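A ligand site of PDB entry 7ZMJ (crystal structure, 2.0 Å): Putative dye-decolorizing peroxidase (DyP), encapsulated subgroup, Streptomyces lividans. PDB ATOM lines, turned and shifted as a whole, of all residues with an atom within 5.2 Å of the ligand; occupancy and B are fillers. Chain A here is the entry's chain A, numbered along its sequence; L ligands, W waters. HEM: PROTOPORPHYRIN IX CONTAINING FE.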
ATOM      1  N   ASP A 140       1.473 -29.453 -25.125  1.00  0.00           N
ATOM      2  CA  ASP A 140       0.222 -28.725 -25.426  1.00  0.00           C
ATOM      3  C   ASP A 140       0.387 -28.179 -26.844  1.00  0.00           C
ATOM      4  O   ASP A 140       1.450 -28.378 -27.466  1.00  0.00           O
ATOM      5  CB  ASP A 140      -0.063 -27.670 -24.369  1.00  0.00           C
ATOM      6  CG  ASP A 140       0.990 -26.621 -24.201  1.00  0.00           C
ATOM      7  OD1 ASP A 140       1.669 -26.289 -25.236  1.00  0.00           O
ATOM      8  OD2 ASP A 140       1.152 -26.126 -23.022  1.00  0.00           O
ATOM      9  N   LEU A 142       0.947 -25.292 -27.898  1.00  0.00           N
ATOM     10  CA  LEU A 142       2.051 -24.313 -28.078  1.00  0.00           C
ATOM     11  C   LEU A 142       3.408 -25.031 -28.220  1.00  0.00           C
ATOM     12  O   LEU A 142       4.404 -24.326 -28.447  1.00  0.00           O
ATOM     13  CB  LEU A 142       2.054 -23.352 -26.872  1.00  0.00           C
ATOM     14  CG  LEU A 142       0.773 -22.537 -26.701  1.00  0.00           C
ATOM     15  CD1 LEU A 142       0.912 -21.565 -25.542  1.00  0.00           C
ATOM     16  CD2 LEU A 142       0.409 -21.801 -27.982  1.00  0.00           C
ATOM     17  N   PHE A 144       4.945 -26.821 -25.857  1.00  0.00           N
ATOM     18  CA  PHE A 144       5.615 -26.940 -24.533  1.00  0.00           C
ATOM     19  C   PHE A 144       5.068 -28.135 -23.760  1.00  0.00           C
ATOM     20  O   PHE A 144       3.833 -28.405 -23.799  1.00  0.00           O
ATOM     21  CB  PHE A 144       5.479 -25.636 -23.737  1.00  0.00           C
ATOM     22  CG  PHE A 144       6.444 -24.557 -24.157  1.00  0.00           C
ATOM     23  CD1 PHE A 144       6.296 -23.902 -25.369  1.00  0.00           C
ATOM     24  CD2 PHE A 144       7.552 -24.262 -23.378  1.00  0.00           C
ATOM     25  CE1 PHE A 144       7.191 -22.939 -25.770  1.00  0.00           C
ATOM     26  CE2 PHE A 144       8.446 -23.300 -23.779  1.00  0.00           C
ATOM     27  CZ  PHE A 144       8.263 -22.623 -24.972  1.00  0.00           C
ATOM     28  N   VAL A 145       5.932 -28.790 -22.983  1.00  0.00           N
ATOM     29  CA  VAL A 145       5.525 -29.833 -22.005  1.00  0.00           C
ATOM     30  C   VAL A 145       4.625 -29.138 -20.994  1.00  0.00           C
ATOM     31  O   VAL A 145       4.957 -28.058 -20.508  1.00  0.00           O
ATOM     32  CB  VAL A 145       6.714 -30.534 -21.331  1.00  0.00           C
ATOM     33  CG1 VAL A 145       6.252 -31.552 -20.331  1.00  0.00           C
ATOM     34  CG2 VAL A 145       7.640 -31.169 -22.344  1.00  0.00           C
ATOM     35  N   ASP A 146       3.530 -29.800 -20.643  1.00  0.00           N
ATOM     36  CA  ASP A 146       2.428 -29.269 -19.842  1.00  0.00           C
ATOM     37  C   ASP A 146       2.086 -30.271 -18.731  1.00  0.00           C
ATOM     38  O   ASP A 146       1.628 -31.342 -19.055  1.00  0.00           O
ATOM     39  CB  ASP A 146       1.265 -29.031 -20.821  1.00  0.00           C
ATOM     40  CG  ASP A 146       0.220 -28.133 -20.297  1.00  0.00           C
ATOM     41  OD1 ASP A 146      -0.086 -28.255 -19.099  1.00  0.00           O
ATOM     42  OD2 ASP A 146      -0.294 -27.305 -21.099  1.00  0.00           O
ATOM     43  N   GLY A 147       2.241 -29.893 -17.460  1.00  0.00           N
ATOM     44  CA  GLY A 147       1.866 -30.673 -16.253  1.00  0.00           C
ATOM     45  C   GLY A 147       3.062 -30.906 -15.328  1.00  0.00           C
ATOM     46  O   GLY A 147       2.853 -31.448 -14.201  1.00  0.00           O
ATOM     47  N   THR A 148       4.273 -30.506 -15.734  1.00  0.00           N
ATOM     48  CA  THR A 148       5.553 -30.830 -15.063  1.00  0.00           C
ATOM     49  C   THR A 148       5.488 -30.578 -13.540  1.00  0.00           C
ATOM     50  O   THR A 148       5.877 -31.452 -12.791  1.00  0.00           O
ATOM     51  CB  THR A 148       6.708 -30.046 -15.697  1.00  0.00           C
ATOM     52  OG1 THR A 148       6.671 -30.274 -17.100  1.00  0.00           O
ATOM     53  CG2 THR A 148       8.070 -30.484 -15.203  1.00  0.00           C
ATOM     54  N   GLU A 149       5.060 -29.398 -13.107  1.00  0.00           N
ATOM     55  CA  GLU A 149       5.152 -28.967 -11.684  1.00  0.00           C
ATOM     56  C   GLU A 149       3.873 -29.286 -10.916  1.00  0.00           C
ATOM     57  O   GLU A 149       3.774 -28.767  -9.738  1.00  0.00           O
ATOM     58  CB  GLU A 149       5.524 -27.484 -11.610  1.00  0.00           C
ATOM     59  CG  GLU A 149       6.980 -27.247 -12.028  1.00  0.00           C
ATOM     60  CD  GLU A 149       7.972 -27.897 -11.082  1.00  0.00           C
ATOM     61  OE1 GLU A 149       7.882 -27.607  -9.887  1.00  0.00           O
ATOM     62  OE2 GLU A 149       8.772 -28.759 -11.505  1.00  0.00           O
ATOM     63  N   ASN A 150       2.950 -30.117 -11.450  1.00  0.00           N
ATOM     64  CA  ASN A 150       1.781 -30.531 -10.632  1.00  0.00           C
ATOM     65  C   ASN A 150       2.254 -31.201  -9.343  1.00  0.00           C
ATOM     66  O   ASN A 150       3.146 -32.026  -9.392  1.00  0.00           O
ATOM     67  CB  ASN A 150       0.843 -31.476 -11.381  1.00  0.00           C
ATOM     68  CG  ASN A 150      -0.190 -30.721 -12.199  1.00  0.00           C
ATOM     69  OD1 ASN A 150      -0.608 -29.623 -11.835  1.00  0.00           O
ATOM     70  ND2 ASN A 150      -0.566 -31.300 -13.314  1.00  0.00           N
ATOM     71  N   GLN A 178     -11.699 -23.605 -18.167  1.00  0.00           N
ATOM     72  CA  GLN A 178     -11.663 -22.580 -19.232  1.00  0.00           C
ATOM     73  C   GLN A 178     -11.211 -23.261 -20.518  1.00  0.00           C
ATOM     74  O   GLN A 178     -10.162 -23.931 -20.518  1.00  0.00           O
ATOM     75  CB  GLN A 178     -10.701 -21.441 -18.922  1.00  0.00           C
ATOM     76  CG  GLN A 178     -10.981 -20.658 -17.650  1.00  0.00           C
ATOM     77  CD  GLN A 178      -9.920 -19.607 -17.493  1.00  0.00           C
ATOM     78  OE1 GLN A 178      -8.761 -19.897 -17.230  1.00  0.00           O
ATOM     79  NE2 GLN A 178     -10.269 -18.346 -17.723  1.00  0.00           N
ATOM     80  N   TYR A 180      -9.574 -22.701 -23.948  1.00  0.00           N
ATOM     81  CA  TYR A 180      -8.706 -21.700 -24.615  1.00  0.00           C
ATOM     82  C   TYR A 180      -8.505 -22.103 -26.073  1.00  0.00           C
ATOM     83  O   TYR A 180      -8.225 -23.279 -26.351  1.00  0.00           O
ATOM     84  CB  TYR A 180      -7.363 -21.589 -23.902  1.00  0.00           C
ATOM     85  CG  TYR A 180      -7.378 -20.813 -22.616  1.00  0.00           C
ATOM     86  CD1 TYR A 180      -7.156 -19.448 -22.575  1.00  0.00           C
ATOM     87  CD2 TYR A 180      -7.495 -21.463 -21.409  1.00  0.00           C
ATOM     88  CE1 TYR A 180      -7.121 -18.745 -21.380  1.00  0.00           C
ATOM     89  CE2 TYR A 180      -7.439 -20.787 -20.191  1.00  0.00           C
ATOM     90  CZ  TYR A 180      -7.253 -19.421 -20.186  1.00  0.00           C
ATOM     91  OH  TYR A 180      -7.240 -18.701 -19.016  1.00  0.00           O
ATOM     92  N   HIS A 182      -5.936 -20.970 -29.325  1.00  0.00           N
ATOM     93  CA  HIS A 182      -4.605 -20.361 -29.492  1.00  0.00           C
ATOM     94  C   HIS A 182      -4.535 -19.705 -30.877  1.00  0.00           C
ATOM     95  O   HIS A 182      -5.057 -20.285 -31.818  1.00  0.00           O
ATOM     96  CB  HIS A 182      -3.493 -21.391 -29.290  1.00  0.00           C
ATOM     97  CG  HIS A 182      -3.453 -21.899 -27.892  1.00  0.00           C
ATOM     98  ND1 HIS A 182      -3.158 -21.056 -26.820  1.00  0.00           N
ATOM     99  CD2 HIS A 182      -3.669 -23.133 -27.387  1.00  0.00           C
ATOM    100  CE1 HIS A 182      -3.205 -21.783 -25.698  1.00  0.00           C
ATOM    101  NE2 HIS A 182      -3.511 -23.058 -26.019  1.00  0.00           N
ATOM    102  N   ILE A 199       6.658 -18.459 -21.616  1.00  0.00           N
ATOM    103  CA  ILE A 199       6.279 -19.582 -20.729  1.00  0.00           C
ATOM    104  C   ILE A 199       7.078 -19.500 -19.425  1.00  0.00           C
ATOM    105  O   ILE A 199       6.485 -19.656 -18.349  1.00  0.00           O
ATOM    106  CB  ILE A 199       6.474 -20.930 -21.439  1.00  0.00           C
ATOM    107  CG1 ILE A 199       5.645 -21.032 -22.722  1.00  0.00           C
ATOM    108  CG2 ILE A 199       6.191 -22.097 -20.491  1.00  0.00           C
ATOM    109  CD1 ILE A 199       4.166 -20.973 -22.523  1.00  0.00           C
ATOM    110  N   ARG A 201      10.050 -21.547 -19.264  1.00  0.00           N
ATOM    111  CA  ARG A 201      10.791 -22.844 -19.308  1.00  0.00           C
ATOM    112  C   ARG A 201      11.392 -23.014 -20.704  1.00  0.00           C
ATOM    113  O   ARG A 201      10.851 -22.424 -21.649  1.00  0.00           O
ATOM    114  CB  ARG A 201       9.903 -24.043 -18.962  1.00  0.00           C
ATOM    115  CG  ARG A 201       9.057 -23.891 -17.692  1.00  0.00           C
ATOM    116  CD  ARG A 201       8.258 -25.123 -17.343  1.00  0.00           C
ATOM    117  NE  ARG A 201       9.126 -26.201 -16.912  1.00  0.00           N
ATOM    118  CZ  ARG A 201       9.454 -26.469 -15.652  1.00  0.00           C
ATOM    119  NH1 ARG A 201       8.917 -25.813 -14.636  1.00  0.00           N
ATOM    120  NH2 ARG A 201      10.323 -27.430 -15.425  1.00  0.00           N
ATOM    121  N   ASP A 206      12.393 -28.664 -21.219  1.00  0.00           N
ATOM    122  CA  ASP A 206      11.440 -28.431 -20.104  1.00  0.00           C
ATOM    123  C   ASP A 206      12.186 -28.063 -18.811  1.00  0.00           C
ATOM    124  O   ASP A 206      11.596 -28.199 -17.731  1.00  0.00           O
ATOM    125  CB  ASP A 206      10.570 -29.675 -19.871  1.00  0.00           C
ATOM    126  CG  ASP A 206       9.346 -29.388 -19.037  1.00  0.00           C
ATOM    127  OD1 ASP A 206       8.892 -28.227 -19.016  1.00  0.00           O
ATOM    128  OD2 ASP A 206       8.904 -30.302 -18.370  1.00  0.00           O
ATOM    129  N   GLU A 208      13.256 -25.278 -16.226  1.00  0.00           N
ATOM    130  CA  GLU A 208      12.824 -23.934 -15.794  1.00  0.00           C
ATOM    131  C   GLU A 208      13.947 -22.908 -16.080  1.00  0.00           C
ATOM    132  O   GLU A 208      15.120 -23.272 -15.875  1.00  0.00           O
ATOM    133  CB  GLU A 208      12.459 -23.963 -14.313  1.00  0.00           C
ATOM    134  CG  GLU A 208      11.720 -22.697 -13.905  1.00  0.00           C
ATOM    135  CD  GLU A 208      11.145 -22.754 -12.515  1.00  0.00           C
ATOM    136  OE1 GLU A 208      11.197 -23.838 -11.894  1.00  0.00           O
ATOM    137  OE2 GLU A 208      10.639 -21.728 -12.080  1.00  0.00           O
ATOM    138  N   HIS A 219       4.438 -16.875 -17.830  1.00  0.00           N
ATOM    139  CA  HIS A 219       3.336 -17.702 -17.283  1.00  0.00           C
ATOM    140  C   HIS A 219       3.751 -18.321 -15.946  1.00  0.00           C
ATOM    141  O   HIS A 219       2.982 -18.251 -14.978  1.00  0.00           O
ATOM    142  CB  HIS A 219       2.916 -18.753 -18.296  1.00  0.00           C
ATOM    143  CG  HIS A 219       1.778 -19.589 -17.848  1.00  0.00           C
ATOM    144  ND1 HIS A 219       0.559 -19.050 -17.543  1.00  0.00           N
ATOM    145  CD2 HIS A 219       1.674 -20.891 -17.688  1.00  0.00           C
ATOM    146  CE1 HIS A 219      -0.286 -19.983 -17.235  1.00  0.00           C
ATOM    147  NE2 HIS A 219       0.391 -21.164 -17.311  1.00  0.00           N
ATOM    148  N   VAL A 220       4.928 -18.916 -15.887  1.00  0.00           N
ATOM    149  CA  VAL A 220       5.464 -19.561 -14.674  1.00  0.00           C
ATOM    150  C   VAL A 220       5.665 -18.541 -13.545  1.00  0.00           C
ATOM    151  O   VAL A 220       5.316 -18.872 -12.411  1.00  0.00           O
ATOM    152  CB  VAL A 220       6.703 -20.411 -15.030  1.00  0.00           C
ATOM    153  CG1 VAL A 220       7.466 -20.842 -13.808  1.00  0.00           C
ATOM    154  CG2 VAL A 220       6.268 -21.630 -15.826  1.00  0.00           C
ATOM    155  N   THR A 223       1.975 -17.472 -12.213  1.00  0.00           N
ATOM    156  CA  THR A 223       1.173 -18.556 -11.590  1.00  0.00           C
ATOM    157  C   THR A 223       1.903 -19.106 -10.365  1.00  0.00           C
ATOM    158  O   THR A 223       1.338 -20.000  -9.718  1.00  0.00           O
ATOM    159  CB  THR A 223       0.809 -19.633 -12.616  1.00  0.00           C
ATOM    160  OG1 THR A 223       2.022 -20.183 -13.148  1.00  0.00           O
ATOM    161  CG2 THR A 223      -0.108 -19.111 -13.709  1.00  0.00           C
ATOM    162  N   SER A 224       3.101 -18.609 -10.063  1.00  0.00           N
ATOM    163  CA  SER A 224       3.858 -18.940  -8.821  1.00  0.00           C
ATOM    164  C   SER A 224       3.397 -17.982  -7.718  1.00  0.00           C
ATOM    165  O   SER A 224       3.708 -16.797  -7.835  1.00  0.00           O
ATOM    166  CB  SER A 224       5.372 -18.850  -9.028  1.00  0.00           C
ATOM    167  OG  SER A 224       5.751 -19.809  -9.997  1.00  0.00           O
ATOM    168  N   ILE A 235      -2.089 -25.832  -7.282  1.00  0.00           N
ATOM    169  CA  ILE A 235      -3.310 -26.453  -7.851  1.00  0.00           C
ATOM    170  C   ILE A 235      -2.887 -27.713  -8.595  1.00  0.00           C
ATOM    171  O   ILE A 235      -1.726 -27.835  -8.897  1.00  0.00           O
ATOM    172  CB  ILE A 235      -4.063 -25.446  -8.741  1.00  0.00           C
ATOM    173  CG1 ILE A 235      -3.302 -25.134 -10.026  1.00  0.00           C
ATOM    174  CG2 ILE A 235      -4.396 -24.200  -7.929  1.00  0.00           C
ATOM    175  CD1 ILE A 235      -4.151 -24.437 -11.065  1.00  0.00           C
ATOM    176  N   ASN A 239      -4.596 -30.016 -18.105  1.00  0.00           N
ATOM    177  CA  ASN A 239      -4.716 -29.451 -19.471  1.00  0.00           C
ATOM    178  C   ASN A 239      -4.753 -30.543 -20.543  1.00  0.00           C
ATOM    179  O   ASN A 239      -3.920 -31.432 -20.534  1.00  0.00           O
ATOM    180  CB  ASN A 239      -3.596 -28.480 -19.799  1.00  0.00           C
ATOM    181  CG  ASN A 239      -3.655 -27.263 -18.906  1.00  0.00           C
ATOM    182  OD1 ASN A 239      -4.470 -27.157 -17.997  1.00  0.00           O
ATOM    183  ND2 ASN A 239      -2.734 -26.326 -19.121  1.00  0.00           N
ATOM    184  N   THR A 252      -6.363 -25.498 -25.878  1.00  0.00           N
ATOM    185  CA  THR A 252      -6.020 -26.139 -24.597  1.00  0.00           C
ATOM    186  C   THR A 252      -7.277 -26.097 -23.743  1.00  0.00           C
ATOM    187  O   THR A 252      -7.830 -24.996 -23.534  1.00  0.00           O
ATOM    188  CB  THR A 252      -4.921 -25.374 -23.872  1.00  0.00           C
ATOM    189  OG1 THR A 252      -3.758 -25.376 -24.706  1.00  0.00           O
ATOM    190  CG2 THR A 252      -4.621 -25.951 -22.512  1.00  0.00           C
ATOM    191  N   PHE A 254      -8.348 -26.200 -20.191  1.00  0.00           N
ATOM    192  CA  PHE A 254      -7.786 -26.035 -18.830  1.00  0.00           C
ATOM    193  C   PHE A 254      -8.820 -26.520 -17.817  1.00  0.00           C
ATOM    194  O   PHE A 254      -9.974 -26.082 -17.816  1.00  0.00           O
ATOM    195  CB  PHE A 254      -7.414 -24.578 -18.545  1.00  0.00           C
ATOM    196  CG  PHE A 254      -7.084 -24.347 -17.089  1.00  0.00           C
ATOM    197  CD1 PHE A 254      -5.842 -24.689 -16.581  1.00  0.00           C
ATOM    198  CD2 PHE A 254      -8.003 -23.797 -16.236  1.00  0.00           C
ATOM    199  CE1 PHE A 254      -5.543 -24.496 -15.240  1.00  0.00           C
ATOM    200  CE2 PHE A 254      -7.691 -23.575 -14.892  1.00  0.00           C
ATOM    201  CZ  PHE A 254      -6.475 -23.953 -14.397  1.00  0.00           C
ATOM    202  N   THR A 264      -7.019 -20.703  -7.025  1.00  0.00           N
ATOM    203  CA  THR A 264      -7.160 -20.636  -8.512  1.00  0.00           C
ATOM    204  C   THR A 264      -7.499 -19.213  -8.918  1.00  0.00           C
ATOM    205  O   THR A 264      -6.964 -18.733  -9.936  1.00  0.00           O
ATOM    206  CB  THR A 264      -8.217 -21.630  -9.008  1.00  0.00           C
ATOM    207  OG1 THR A 264      -7.976 -22.875  -8.370  1.00  0.00           O
ATOM    208  CG2 THR A 264      -8.133 -21.849 -10.497  1.00  0.00           C
ATOM    209  N   MET A 267      -4.525 -16.887  -8.912  1.00  0.00           N
ATOM    210  CA  MET A 267      -3.721 -17.124 -10.132  1.00  0.00           C
ATOM    211  C   MET A 267      -4.362 -16.425 -11.341  1.00  0.00           C
ATOM    212  O   MET A 267      -3.624 -15.715 -12.056  1.00  0.00           O
ATOM    213  CB  MET A 267      -3.523 -18.607 -10.405  1.00  0.00           C
ATOM    214  CG  MET A 267      -2.689 -19.275  -9.349  1.00  0.00           C
ATOM    215  SD  MET A 267      -2.584 -21.029  -9.641  1.00  0.00           S
ATOM    216  CE  MET A 267      -1.481 -21.540  -8.335  1.00  0.00           C
ATOM    217  N   LEU A 268      -5.678 -16.566 -11.530  1.00  0.00           N
ATOM    218  CA  LEU A 268      -6.392 -15.924 -12.648  1.00  0.00           C
ATOM    219  C   LEU A 268      -6.298 -14.397 -12.559  1.00  0.00           C
ATOM    220  O   LEU A 268      -6.147 -13.737 -13.615  1.00  0.00           O
ATOM    221  CB  LEU A 268      -7.845 -16.388 -12.642  1.00  0.00           C
ATOM    222  CG  LEU A 268      -8.083 -17.816 -13.145  1.00  0.00           C
ATOM    223  CD1 LEU A 268      -9.524 -18.161 -12.944  1.00  0.00           C
ATOM    224  CD2 LEU A 268      -7.707 -17.950 -14.636  1.00  0.00           C
ATOM    225  N   MET A 271      -2.944 -13.358 -13.758  1.00  0.00           N
ATOM    226  CA  MET A 271      -2.835 -13.553 -15.226  1.00  0.00           C
ATOM    227  C   MET A 271      -3.557 -12.439 -15.987  1.00  0.00           C
ATOM    228  O   MET A 271      -2.963 -11.897 -16.930  1.00  0.00           O
ATOM    229  CB  MET A 271      -3.399 -14.924 -15.633  1.00  0.00           C
ATOM    230  CG  MET A 271      -2.535 -16.089 -15.166  1.00  0.00           C
ATOM    231  SD  MET A 271      -3.320 -17.659 -15.550  1.00  0.00           S
ATOM    232  CE  MET A 271      -3.452 -17.564 -17.331  1.00  0.00           C
ATOM    233  N   ILE A 283       1.191 -15.409 -21.953  1.00  0.00           N
ATOM    234  CA  ILE A 283       0.490 -16.542 -22.625  1.00  0.00           C
ATOM    235  C   ILE A 283      -0.867 -16.065 -23.175  1.00  0.00           C
ATOM    236  O   ILE A 283      -1.285 -16.581 -24.211  1.00  0.00           O
ATOM    237  CB  ILE A 283       0.360 -17.767 -21.698  1.00  0.00           C
ATOM    238  CG1 ILE A 283       0.447 -19.078 -22.479  1.00  0.00           C
ATOM    239  CG2 ILE A 283      -0.888 -17.726 -20.846  1.00  0.00           C
ATOM    240  CD1 ILE A 283       0.559 -20.323 -21.619  1.00  0.00           C
ATOM    241  N   SER A 287      -3.613 -16.715 -26.551  1.00  0.00           N
ATOM    242  CA  SER A 287      -4.634 -17.612 -25.956  1.00  0.00           C
ATOM    243  C   SER A 287      -5.860 -16.790 -25.565  1.00  0.00           C
ATOM    244  O   SER A 287      -5.706 -15.912 -24.713  1.00  0.00           O
ATOM    245  CB  SER A 287      -4.091 -18.357 -24.762  1.00  0.00           C
ATOM    246  OG  SER A 287      -2.784 -18.837 -24.997  1.00  0.00           O
HETATM  247  CHA HEM L   1       2.523 -24.170 -15.605  1.00  0.00           C
HETATM  248  CHB HEM L   1       0.564 -24.030 -20.026  1.00  0.00           C
HETATM  249  CHC HEM L   1      -3.447 -21.895 -18.277  1.00  0.00           C
HETATM  250  CHD HEM L   1      -1.634 -22.443 -13.861  1.00  0.00           C
HETATM  251  C1A HEM L   1       2.343 -24.273 -16.965  1.00  0.00           C
HETATM  252  C2A HEM L   1       3.371 -24.709 -17.851  1.00  0.00           C
HETATM  253  C3A HEM L   1       2.826 -24.646 -19.121  1.00  0.00           C
HETATM  254  C4A HEM L   1       1.441 -24.236 -19.012  1.00  0.00           C
HETATM  255  CMA HEM L   1       3.475 -25.029 -20.388  1.00  0.00           C
HETATM  256  CAA HEM L   1       4.786 -25.120 -17.492  1.00  0.00           C
HETATM  257  CBA HEM L   1       4.902 -26.612 -17.172  1.00  0.00           C
HETATM  258  CGA HEM L   1       4.138 -27.034 -15.958  1.00  0.00           C
HETATM  259  O1A HEM L   1       2.951 -27.431 -16.129  1.00  0.00           O
HETATM  260  O2A HEM L   1       4.664 -26.943 -14.790  1.00  0.00           O
HETATM  261  C1B HEM L   1      -0.700 -23.430 -19.929  1.00  0.00           C
HETATM  262  C2B HEM L   1      -1.548 -23.190 -21.042  1.00  0.00           C
HETATM  263  C3B HEM L   1      -2.743 -22.661 -20.578  1.00  0.00           C
HETATM  264  C4B HEM L   1      -2.531 -22.485 -19.126  1.00  0.00           C
HETATM  265  CMB HEM L   1      -1.228 -23.596 -22.516  1.00  0.00           C
HETATM  266  CAB HEM L   1      -3.729 -22.135 -21.527  1.00  0.00           C
HETATM  267  CBB HEM L   1      -3.988 -20.854 -21.519  1.00  0.00           C
HETATM  268  C1C HEM L   1      -3.336 -21.772 -16.914  1.00  0.00           C
HETATM  269  C2C HEM L   1      -4.299 -21.248 -15.999  1.00  0.00           C
HETATM  270  C3C HEM L   1      -3.732 -21.372 -14.744  1.00  0.00           C
HETATM  271  C4C HEM L   1      -2.466 -22.065 -14.900  1.00  0.00           C
HETATM  272  CMC HEM L   1      -5.603 -20.623 -16.374  1.00  0.00           C
HETATM  273  CAC HEM L   1      -4.246 -21.049 -13.414  1.00  0.00           C
HETATM  274  CBC HEM L   1      -5.401 -20.532 -13.213  1.00  0.00           C
HETATM  275  C1D HEM L   1      -0.375 -22.967 -14.046  1.00  0.00           C
HETATM  276  C2D HEM L   1       0.527 -23.242 -12.885  1.00  0.00           C
HETATM  277  C3D HEM L   1       1.698 -23.706 -13.355  1.00  0.00           C
HETATM  278  C4D HEM L   1       1.507 -23.702 -14.796  1.00  0.00           C
HETATM  279  CMD HEM L   1       0.193 -23.070 -11.412  1.00  0.00           C
HETATM  280  CAD HEM L   1       2.894 -24.109 -12.513  1.00  0.00           C
HETATM  281  CBD HEM L   1       3.825 -22.941 -12.224  1.00  0.00           C
HETATM  282  CGD HEM L   1       4.926 -23.488 -11.305  1.00  0.00           C
HETATM  283  O1D HEM L   1       4.629 -23.576 -10.070  1.00  0.00           O
HETATM  284  O2D HEM L   1       6.014 -23.950 -11.783  1.00  0.00           O
HETATM  285  NA  HEM L   1       1.197 -23.993 -17.662  1.00  0.00           N
HETATM  286  NB  HEM L   1      -1.307 -22.960 -18.846  1.00  0.00           N
HETATM  287  NC  HEM L   1      -2.270 -22.305 -16.233  1.00  0.00           N
HETATM  288  ND  HEM L   1       0.239 -23.295 -15.185  1.00  0.00           N
HETATM  289 FE   HEM L   1      -0.474 -23.113 -16.965  1.00  0.00          FE
HETATM  290  O   HOH W   1      -1.330 -25.143 -16.635  1.00  0.00           O
HETATM  291  O   HOH W   2       2.523 -22.893  -9.023  1.00  0.00           O
HETATM  292  O   HOH W   3       0.170 -27.052 -16.681  1.00  0.00           O
HETATM  293  O   HOH W   4       6.284 -24.880 -14.344  1.00  0.00           O
HETATM  294  O   HOH W   5       1.758 -27.752 -13.546  1.00  0.00           O
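Merely in contact with the ligand: Asp 140, Phe 144, Val 145, Asp 146, Gln 178, Tyr 180, Ile 199, Arg 201, Val 220, Thr 223, Ser 224, Asn 239, Thr 252, Phe 254, Met 267, Leu 268, Met 271 and Ile 283.
22 residues have an atom within 4 Å of the ligand: Asp 140, Phe 144, Val 145, Asp 146, Gly 147, Thr 148, Glu 149, Gln 178, Tyr 180, Ile 199, Arg 201, His 219, Val 220, Thr 223, Ser 224, Asn 239, Thr 252, Phe 254, Met 267, Leu 268, Met 271 and Ile 283.
The backbone carbonyl oxygen of His 219 is in hydrogen-bond range of the side-chain hydroxyl of Thr 223, 2.8 Å away.
O of Ile 199 is in hydrogen-bond range of N of His 219 (3.5 Å).
O of Gln 178 is in hydrogen-bond range of N of Phe 254 (2.9 Å).
OD2 of Asp 206 sits at hydrogen-bond distance from OG1 of Thr 148.
OD1 of Asp 140 lies within hydrogen-bond range of N of Leu 142, at 2.9 Å.
The side-chain amide nitrogen of Asn 239 sits at hydrogen-bond distance from the side-chain carboxylate of Asp 146.
The backbone NH (N) of Tyr 180 is in hydrogen-bond range of the backbone carbonyl oxygen (O) of Thr 252, 2.9 Å away.
O of Val 220 sits at hydrogen-bond distance from OG of Ser 224 (2.6 Å).
A ring nitrogen (NE2) of His 219 binds an iron atom (FE) of the ligand (2.2 Å).
The backbone NH (N) of Gly 147 lies within hydrogen-bond range of an oxygen (O1A) of the ligand.
The backbone NH (N) of Glu 149 sits at hydrogen-bond distance from an oxygen (O2A) of the ligand, 3.0 Å away.
N of Thr 148 is in hydrogen-bond range of O1A of the ligand (3.4 Å).
Water W2 bridges O1D of the ligand and O of Thr 223.
Water W4 lies within hydrogen-bond range of O2A of the ligand and NH1 of Arg 201.
Water W3 lies within hydrogen-bond range of the side-chain carboxylate (OD1) of Asp 146 and an oxygen (O1A) of the ligand.
Water W5 bridges O1A of the ligand (2.9 Å) and N of Asn 150 (3.4 Å).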
